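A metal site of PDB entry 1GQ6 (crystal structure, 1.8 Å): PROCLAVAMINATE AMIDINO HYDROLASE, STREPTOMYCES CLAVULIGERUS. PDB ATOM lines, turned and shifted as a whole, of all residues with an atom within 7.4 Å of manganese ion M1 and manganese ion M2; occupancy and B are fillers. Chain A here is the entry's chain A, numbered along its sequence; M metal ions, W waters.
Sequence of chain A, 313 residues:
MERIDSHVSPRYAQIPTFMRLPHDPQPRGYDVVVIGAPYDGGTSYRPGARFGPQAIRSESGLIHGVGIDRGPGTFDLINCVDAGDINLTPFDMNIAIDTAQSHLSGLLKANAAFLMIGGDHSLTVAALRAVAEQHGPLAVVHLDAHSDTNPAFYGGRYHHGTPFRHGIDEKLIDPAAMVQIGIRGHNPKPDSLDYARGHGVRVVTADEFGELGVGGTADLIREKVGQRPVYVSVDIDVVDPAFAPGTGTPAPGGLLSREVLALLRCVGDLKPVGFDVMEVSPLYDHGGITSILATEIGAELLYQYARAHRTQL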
ATOM      1  N   ASP A 120     -12.269  24.377  16.316  1.00  0.00           N
ATOM      2  CA  ASP A 120     -11.227  23.721  15.545  1.00  0.00           C
ATOM      3  C   ASP A 120     -11.671  23.351  14.141  1.00  0.00           C
ATOM      4  O   ASP A 120     -12.858  23.280  13.863  1.00  0.00           O
ATOM      5  CB  ASP A 120     -10.596  22.572  16.311  1.00  0.00           C
ATOM      6  CG  ASP A 120     -11.410  21.312  16.273  1.00  0.00           C
ATOM      7  OD1 ASP A 120     -11.485  20.661  15.195  1.00  0.00           O
ATOM      8  OD2 ASP A 120     -11.969  20.911  17.311  1.00  0.00           O
ATOM      9  N   HIS A 121     -10.709  23.125  13.265  1.00  0.00           N
ATOM     10  CA  HIS A 121     -10.972  22.955  11.846  1.00  0.00           C
ATOM     11  C   HIS A 121     -11.805  21.719  11.489  1.00  0.00           C
ATOM     12  O   HIS A 121     -12.361  21.654  10.402  1.00  0.00           O
ATOM     13  CB  HIS A 121      -9.633  22.960  11.077  1.00  0.00           C
ATOM     14  CG  HIS A 121      -9.657  23.751   9.823  1.00  0.00           C
ATOM     15  ND1 HIS A 121      -8.505  24.220   9.222  1.00  0.00           N
ATOM     16  CD2 HIS A 121     -10.700  24.153   9.047  1.00  0.00           C
ATOM     17  CE1 HIS A 121      -8.843  24.901   8.143  1.00  0.00           C
ATOM     18  NE2 HIS A 121     -10.158  24.851   7.997  1.00  0.00           N
ATOM     19  N   SER A 122     -11.902  20.747  12.382  1.00  0.00           N
ATOM     20  CA  SER A 122     -12.720  19.561  12.068  1.00  0.00           C
ATOM     21  C   SER A 122     -14.131  19.935  11.724  1.00  0.00           C
ATOM     22  O   SER A 122     -14.764  19.255  10.959  1.00  0.00           O
ATOM     23  CB  SER A 122     -12.751  18.588  13.238  1.00  0.00           C
ATOM     24  OG  SER A 122     -13.329  19.149  14.408  1.00  0.00           O
ATOM     25  N   HIS A 142      -8.549  27.231   0.622  1.00  0.00           N
ATOM     26  CA  HIS A 142      -8.197  26.794   1.970  1.00  0.00           C
ATOM     27  C   HIS A 142      -6.872  27.437   2.331  1.00  0.00           C
ATOM     28  O   HIS A 142      -5.877  27.196   1.654  1.00  0.00           O
ATOM     29  CB  HIS A 142      -8.115  25.271   1.997  1.00  0.00           C
ATOM     30  CG  HIS A 142      -7.565  24.675   3.264  1.00  0.00           C
ATOM     31  ND1 HIS A 142      -6.811  23.518   3.258  1.00  0.00           N
ATOM     32  CD2 HIS A 142      -7.718  25.010   4.569  1.00  0.00           C
ATOM     33  CE1 HIS A 142      -6.469  23.201   4.488  1.00  0.00           C
ATOM     34  NE2 HIS A 142      -7.015  24.082   5.311  1.00  0.00           N
ATOM     35  N   LEU A 143      -6.860  28.271   3.386  1.00  0.00           N
ATOM     36  CA  LEU A 143      -5.621  28.924   3.846  1.00  0.00           C
ATOM     37  C   LEU A 143      -5.250  28.231   5.148  1.00  0.00           C
ATOM     38  O   LEU A 143      -6.043  28.184   6.082  1.00  0.00           O
ATOM     39  CB  LEU A 143      -5.817  30.407   4.139  1.00  0.00           C
ATOM     40  CG  LEU A 143      -6.316  31.288   2.984  1.00  0.00           C
ATOM     41  CD1 LEU A 143      -6.052  32.765   3.353  1.00  0.00           C
ATOM     42  CD2 LEU A 143      -5.736  30.950   1.699  1.00  0.00           C
ATOM     43  N   ASP A 144      -4.023  27.723   5.218  1.00  0.00           N
ATOM     44  CA  ASP A 144      -3.602  26.891   6.333  1.00  0.00           C
ATOM     45  C   ASP A 144      -2.096  26.623   6.270  1.00  0.00           C
ATOM     46  O   ASP A 144      -1.508  26.600   5.199  1.00  0.00           O
ATOM     47  CB  ASP A 144      -4.313  25.540   6.199  1.00  0.00           C
ATOM     48  CG  ASP A 144      -4.568  24.855   7.545  1.00  0.00           C
ATOM     49  OD1 ASP A 144      -3.651  24.751   8.359  1.00  0.00           O
ATOM     50  OD2 ASP A 144      -5.657  24.372   7.855  1.00  0.00           O
ATOM     51  N   ALA A 145      -1.462  26.405   7.431  1.00  0.00           N
ATOM     52  CA  ALA A 145      -0.091  25.927   7.436  1.00  0.00           C
ATOM     53  C   ALA A 145      -0.037  24.440   7.196  1.00  0.00           C
ATOM     54  O   ALA A 145       1.049  23.902   6.931  1.00  0.00           O
ATOM     55  CB  ALA A 145       0.541  26.189   8.774  1.00  0.00           C
ATOM     56  N   HIS A 146      -1.194  23.783   7.318  1.00  0.00           N
ATOM     57  CA  HIS A 146      -1.284  22.311   7.224  1.00  0.00           C
ATOM     58  C   HIS A 146      -2.352  21.927   6.209  1.00  0.00           C
ATOM     59  O   HIS A 146      -3.352  22.599   6.073  1.00  0.00           O
ATOM     60  CB  HIS A 146      -1.687  21.761   8.590  1.00  0.00           C
ATOM     61  CG  HIS A 146      -0.934  22.364   9.717  1.00  0.00           C
ATOM     62  ND1 HIS A 146      -1.396  23.461  10.404  1.00  0.00           N
ATOM     63  CD2 HIS A 146       0.272  22.059  10.236  1.00  0.00           C
ATOM     64  CE1 HIS A 146      -0.509  23.791  11.332  1.00  0.00           C
ATOM     65  NE2 HIS A 146       0.511  22.964  11.240  1.00  0.00           N
ATOM     66  N   SER A 147      -2.143  20.806   5.518  1.00  0.00           N
ATOM     67  CA  SER A 147      -3.045  20.372   4.456  1.00  0.00           C
ATOM     68  C   SER A 147      -4.407  19.894   4.961  1.00  0.00           C
ATOM     69  O   SER A 147      -5.404  20.054   4.272  1.00  0.00           O
ATOM     70  CB  SER A 147      -2.393  19.275   3.639  1.00  0.00           C
ATOM     71  OG  SER A 147      -3.243  18.859   2.609  1.00  0.00           O
ATOM     72  N   ASP A 148      -4.438  19.296   6.148  1.00  0.00           N
ATOM     73  CA  ASP A 148      -5.683  18.823   6.750  1.00  0.00           C
ATOM     74  C   ASP A 148      -6.417  17.817   5.831  1.00  0.00           C
ATOM     75  O   ASP A 148      -7.663  17.804   5.738  1.00  0.00           O
ATOM     76  CB  ASP A 148      -6.619  19.962   7.140  1.00  0.00           C
ATOM     77  CG  ASP A 148      -6.096  20.812   8.288  1.00  0.00           C
ATOM     78  OD1 ASP A 148      -5.027  20.520   8.875  1.00  0.00           O
ATOM     79  OD2 ASP A 148      -6.720  21.767   8.681  1.00  0.00           O
ATOM     80  N   HIS A 160      -8.814  17.228  13.788  1.00  0.00           N
ATOM     81  CA  HIS A 160      -8.750  18.444  12.993  1.00  0.00           C
ATOM     82  C   HIS A 160      -7.849  18.407  11.787  1.00  0.00           C
ATOM     83  O   HIS A 160      -7.746  19.382  11.087  1.00  0.00           O
ATOM     84  CB  HIS A 160      -8.468  19.662  13.868  1.00  0.00           C
ATOM     85  CG  HIS A 160      -7.121  19.669  14.508  1.00  0.00           C
ATOM     86  ND1 HIS A 160      -6.542  20.843  14.969  1.00  0.00           N
ATOM     87  CD2 HIS A 160      -6.249  18.683  14.791  1.00  0.00           C
ATOM     88  CE1 HIS A 160      -5.376  20.551  15.522  1.00  0.00           C
ATOM     89  NE2 HIS A 160      -5.170  19.243  15.415  1.00  0.00           N
ATOM     90  N   GLY A 161      -7.213  17.279  11.552  1.00  0.00           N
ATOM     91  CA  GLY A 161      -6.405  17.096  10.366  1.00  0.00           C
ATOM     92  C   GLY A 161      -7.138  16.376   9.258  1.00  0.00           C
ATOM     93  O   GLY A 161      -6.526  16.058   8.215  1.00  0.00           O
ATOM     94  N   PRO A 163     -10.595  17.435   7.818  1.00  0.00           N
ATOM     95  CA  PRO A 163     -11.795  17.952   7.139  1.00  0.00           C
ATOM     96  C   PRO A 163     -11.764  17.908   5.639  1.00  0.00           C
ATOM     97  O   PRO A 163     -12.795  17.573   4.987  1.00  0.00           O
ATOM     98  CB  PRO A 163     -11.898  19.406   7.633  1.00  0.00           C
ATOM     99  CG  PRO A 163     -10.550  19.699   8.154  1.00  0.00           C
ATOM    100  CD  PRO A 163     -10.022  18.429   8.743  1.00  0.00           C
ATOM    101  N   PHE A 164     -10.617  18.211   5.031  1.00  0.00           N
ATOM    102  CA  PHE A 164     -10.590  18.180   3.575  1.00  0.00           C
ATOM    103  C   PHE A 164     -10.461  16.786   2.964  1.00  0.00           C
ATOM    104  O   PHE A 164     -10.781  16.606   1.817  1.00  0.00           O
ATOM    105  CB  PHE A 164      -9.591  19.212   3.042  1.00  0.00           C
ATOM    106  CG  PHE A 164      -9.910  20.586   3.558  1.00  0.00           C
ATOM    107  CD1 PHE A 164     -10.856  21.364   2.944  1.00  0.00           C
ATOM    108  CD2 PHE A 164      -9.340  21.034   4.719  1.00  0.00           C
ATOM    109  CE1 PHE A 164     -11.220  22.575   3.475  1.00  0.00           C
ATOM    110  CE2 PHE A 164      -9.722  22.252   5.262  1.00  0.00           C
ATOM    111  CZ  PHE A 164     -10.639  23.023   4.619  1.00  0.00           C
ATOM    112  N   SER A 233     -12.129  28.630   3.489  1.00  0.00           N
ATOM    113  CA  SER A 233     -11.857  28.177   4.848  1.00  0.00           C
ATOM    114  C   SER A 233     -10.486  28.628   5.294  1.00  0.00           C
ATOM    115  O   SER A 233      -9.482  28.288   4.674  1.00  0.00           O
ATOM    116  CB  SER A 233     -11.966  26.655   4.897  1.00  0.00           C
ATOM    117  OG  SER A 233     -11.767  26.160   6.224  1.00  0.00           O
ATOM    118  N   VAL A 234     -10.445  29.449   6.331  1.00  0.00           N
ATOM    119  CA  VAL A 234      -9.192  29.985   6.818  1.00  0.00           C
ATOM    120  C   VAL A 234      -8.870  29.410   8.190  1.00  0.00           C
ATOM    121  O   VAL A 234      -9.619  29.600   9.141  1.00  0.00           O
ATOM    122  CB  VAL A 234      -9.230  31.524   6.947  1.00  0.00           C
ATOM    123  CG1 VAL A 234      -7.895  32.078   7.378  1.00  0.00           C
ATOM    124  CG2 VAL A 234      -9.679  32.137   5.660  1.00  0.00           C
ATOM    125  N   ASP A 235      -7.726  28.727   8.274  1.00  0.00           N
ATOM    126  CA  ASP A 235      -7.139  28.325   9.556  1.00  0.00           C
ATOM    127  C   ASP A 235      -6.234  29.508   9.937  1.00  0.00           C
ATOM    128  O   ASP A 235      -5.337  29.878   9.194  1.00  0.00           O
ATOM    129  CB  ASP A 235      -6.295  27.049   9.375  1.00  0.00           C
ATOM    130  CG  ASP A 235      -5.756  26.471  10.682  1.00  0.00           C
ATOM    131  OD1 ASP A 235      -5.492  27.222  11.626  1.00  0.00           O
ATOM    132  OD2 ASP A 235      -5.498  25.239  10.794  1.00  0.00           O
ATOM    133  N   ILE A 236      -6.479  30.100  11.089  1.00  0.00           N
ATOM    134  CA  ILE A 236      -5.707  31.254  11.542  1.00  0.00           C
ATOM    135  C   ILE A 236      -4.206  30.949  11.596  1.00  0.00           C
ATOM    136  O   ILE A 236      -3.389  31.881  11.474  1.00  0.00           O
ATOM    137  CB  ILE A 236      -6.257  31.775  12.886  1.00  0.00           C
ATOM    138  CG1 ILE A 236      -5.900  33.264  13.087  1.00  0.00           C
ATOM    139  CG2 ILE A 236      -5.760  30.933  14.072  1.00  0.00           C
ATOM    140  CD1 ILE A 236      -6.582  34.185  12.147  1.00  0.00           C
ATOM    141  N   ASP A 237      -3.844  29.670  11.692  1.00  0.00           N
ATOM    142  CA  ASP A 237      -2.428  29.300  11.768  1.00  0.00           C
ATOM    143  C   ASP A 237      -1.695  29.426  10.426  1.00  0.00           C
ATOM    144  O   ASP A 237      -0.498  29.197  10.346  1.00  0.00           O
ATOM    145  CB  ASP A 237      -2.231  27.931  12.461  1.00  0.00           C
ATOM    146  CG  ASP A 237      -2.608  26.715  11.645  1.00  0.00           C
ATOM    147  OD1 ASP A 237      -2.695  26.782  10.396  1.00  0.00           O
ATOM    148  OD2 ASP A 237      -2.796  25.604  12.251  1.00  0.00           O
ATOM    149  N   VAL A 238      -2.390  29.897   9.393  1.00  0.00           N
ATOM    150  CA  VAL A 238      -1.745  30.173   8.131  1.00  0.00           C
ATOM    151  C   VAL A 238      -0.737  31.334   8.282  1.00  0.00           C
ATOM    152  O   VAL A 238       0.323  31.345   7.610  1.00  0.00           O
ATOM    153  CB  VAL A 238      -2.753  30.470   6.993  1.00  0.00           C
ATOM    154  CG1 VAL A 238      -3.488  31.770   7.264  1.00  0.00           C
ATOM    155  CG2 VAL A 238      -2.023  30.507   5.630  1.00  0.00           C
ATOM    156  N   THR A 247      -3.238  30.002  18.839  1.00  0.00           N
ATOM    157  CA  THR A 247      -3.706  28.910  18.007  1.00  0.00           C
ATOM    158  C   THR A 247      -3.093  27.604  18.510  1.00  0.00           C
ATOM    159  O   THR A 247      -2.068  27.621  19.207  1.00  0.00           O
ATOM    160  CB  THR A 247      -3.441  29.178  16.532  1.00  0.00           C
ATOM    161  OG1 THR A 247      -4.195  28.255  15.727  1.00  0.00           O
ATOM    162  CG2 THR A 247      -1.983  28.978  16.142  1.00  0.00           C
ATOM    163  N   THR A 249      -1.845  24.672  16.875  1.00  0.00           N
ATOM    164  CA  THR A 249      -0.688  24.071  16.269  1.00  0.00           C
ATOM    165  C   THR A 249       0.028  25.121  15.452  1.00  0.00           C
ATOM    166  O   THR A 249      -0.042  25.098  14.218  1.00  0.00           O
ATOM    167  CB  THR A 249      -1.065  22.902  15.355  1.00  0.00           C
ATOM    168  OG1 THR A 249      -2.084  23.308  14.418  1.00  0.00           O
ATOM    169  CG2 THR A 249      -1.654  21.719  16.186  1.00  0.00           C
ATOM    170  N   PRO A 250       0.753  26.009  16.123  1.00  0.00           N
ATOM    171  CA  PRO A 250       1.495  27.037  15.395  1.00  0.00           C
ATOM    172  C   PRO A 250       2.579  26.428  14.554  1.00  0.00           C
ATOM    173  O   PRO A 250       3.106  25.379  14.896  1.00  0.00           O
ATOM    174  CB  PRO A 250       2.149  27.875  16.484  1.00  0.00           C
ATOM    175  CG  PRO A 250       1.476  27.465  17.793  1.00  0.00           C
ATOM    176  CD  PRO A 250       0.911  26.107  17.586  1.00  0.00           C
ATOM    177  N   ALA A 251       2.909  27.125  13.465  1.00  0.00           N
ATOM    178  CA  ALA A 251       3.920  26.690  12.536  1.00  0.00           C
ATOM    179  C   ALA A 251       4.795  27.866  12.131  1.00  0.00           C
ATOM    180  O   ALA A 251       4.348  28.713  11.341  1.00  0.00           O
ATOM    181  CB  ALA A 251       3.263  26.050  11.305  1.00  0.00           C
ATOM    182  N   MET A 278     -11.136  29.519  11.524  1.00  0.00           N
ATOM    183  CA  MET A 278     -10.980  28.482  12.507  1.00  0.00           C
ATOM    184  C   MET A 278      -9.664  28.528  13.268  1.00  0.00           C
ATOM    185  O   MET A 278      -8.695  29.175  12.840  1.00  0.00           O
ATOM    186  CB  MET A 278     -11.103  27.137  11.784  1.00  0.00           C
ATOM    187  CG  MET A 278     -12.303  27.024  10.828  1.00  0.00           C
ATOM    188  SD  MET A 278     -13.854  27.354  11.615  1.00  0.00           S
ATOM    189  CE  MET A 278     -14.234  25.751  12.324  1.00  0.00           C
ATOM    190  N   GLU A 279      -9.663  27.802  14.375  1.00  0.00           N
ATOM    191  CA  GLU A 279      -8.493  27.478  15.191  1.00  0.00           C
ATOM    192  C   GLU A 279      -7.971  28.590  16.079  1.00  0.00           C
ATOM    193  O   GLU A 279      -6.874  28.490  16.627  1.00  0.00           O
ATOM    194  CB  GLU A 279      -7.349  26.825  14.402  1.00  0.00           C
ATOM    195  CG  GLU A 279      -7.725  25.493  13.745  1.00  0.00           C
ATOM    196  CD  GLU A 279      -7.671  24.284  14.660  1.00  0.00           C
ATOM    197  OE1 GLU A 279      -7.450  24.444  15.864  1.00  0.00           O
ATOM    198  OE2 GLU A 279      -7.923  23.188  14.164  1.00  0.00           O
HETATM  199 MN    MN M   1      -6.431  23.538   9.723  1.00  0.00          MN
HETATM  200 MN    MN M   2      -3.360  24.546  10.497  1.00  0.00          MN
HETATM  201  O   HOH W   1      -4.407  22.662  10.519  1.00  0.00           O
HETATM  202  O   HOH W   2      -6.751  22.357  11.595  1.00  0.00           O
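Water W2 bridges OE2 of Glu 279 (2.9 Å) and O of His 160 (3.2 Å).
Four residues have an atom within 4 Å of manganese ion M2: Asp 144, His 146, Asp 235 and Asp 237. Along chain A the residues within 4 Å of manganese ion M2 span positions 144 to 237.
OD2 of Asp 148 binds manganese ion M1. Manganese ion M1 is bound by OD2 of Asp 144 (2.2 Å). OD2 of Asp 235 is bound to manganese ion M1 (2.2 Å). Manganese ion M1 is bound by water W2 (2.2 Å). ND1 of His 121 is bound to manganese ion M1, 2.2 Å away. Manganese ion M1 is bound by water W1 (2.3 Å).
Manganese ion M2 is bound by OD2 of Asp 237 (2.1 Å), water W1 (2.2 Å), OD1 of Asp 144 (2.2 Å), ND1 of His 146 (2.2 Å), OD2 of Asp 235 (2.3 Å) and OD1 of Asp 237 (2.3 Å). Manganese ion M2 has six donor atoms within binding distance.
The side-chain carboxylate (OD1) of Asp 237 sits close to the backbone NH (N) of Ala 145 (3.2 Å). A ring nitrogen (NE2) of His 121 sits at hydrogen-bond distance from the side-chain hydroxyl (OG) of Ser 233, 2.7 Å away. The backbone NH of His 121 lies within hydrogen-bond range of the side-chain carboxylate of Glu 279 (2.9 Å). O of Asp 148 is in hydrogen-bond range of N of Phe 164, 3.1 Å away. OD2 of Asp 237 sits close to OG1 of Thr 249, 3.2 Å away. The side-chain carboxylate of Asp 144 sits close to a ring nitrogen (NE2) of His 142 (2.9 Å). The backbone NH (N) of Asp 235 is in hydrogen-bond range of the backbone carbonyl oxygen (O) of Leu 143 (2.8 Å).
Four residues have an atom within 4 Å of manganese ion M1: His 121, Asp 144, Asp 148 and Asp 235.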
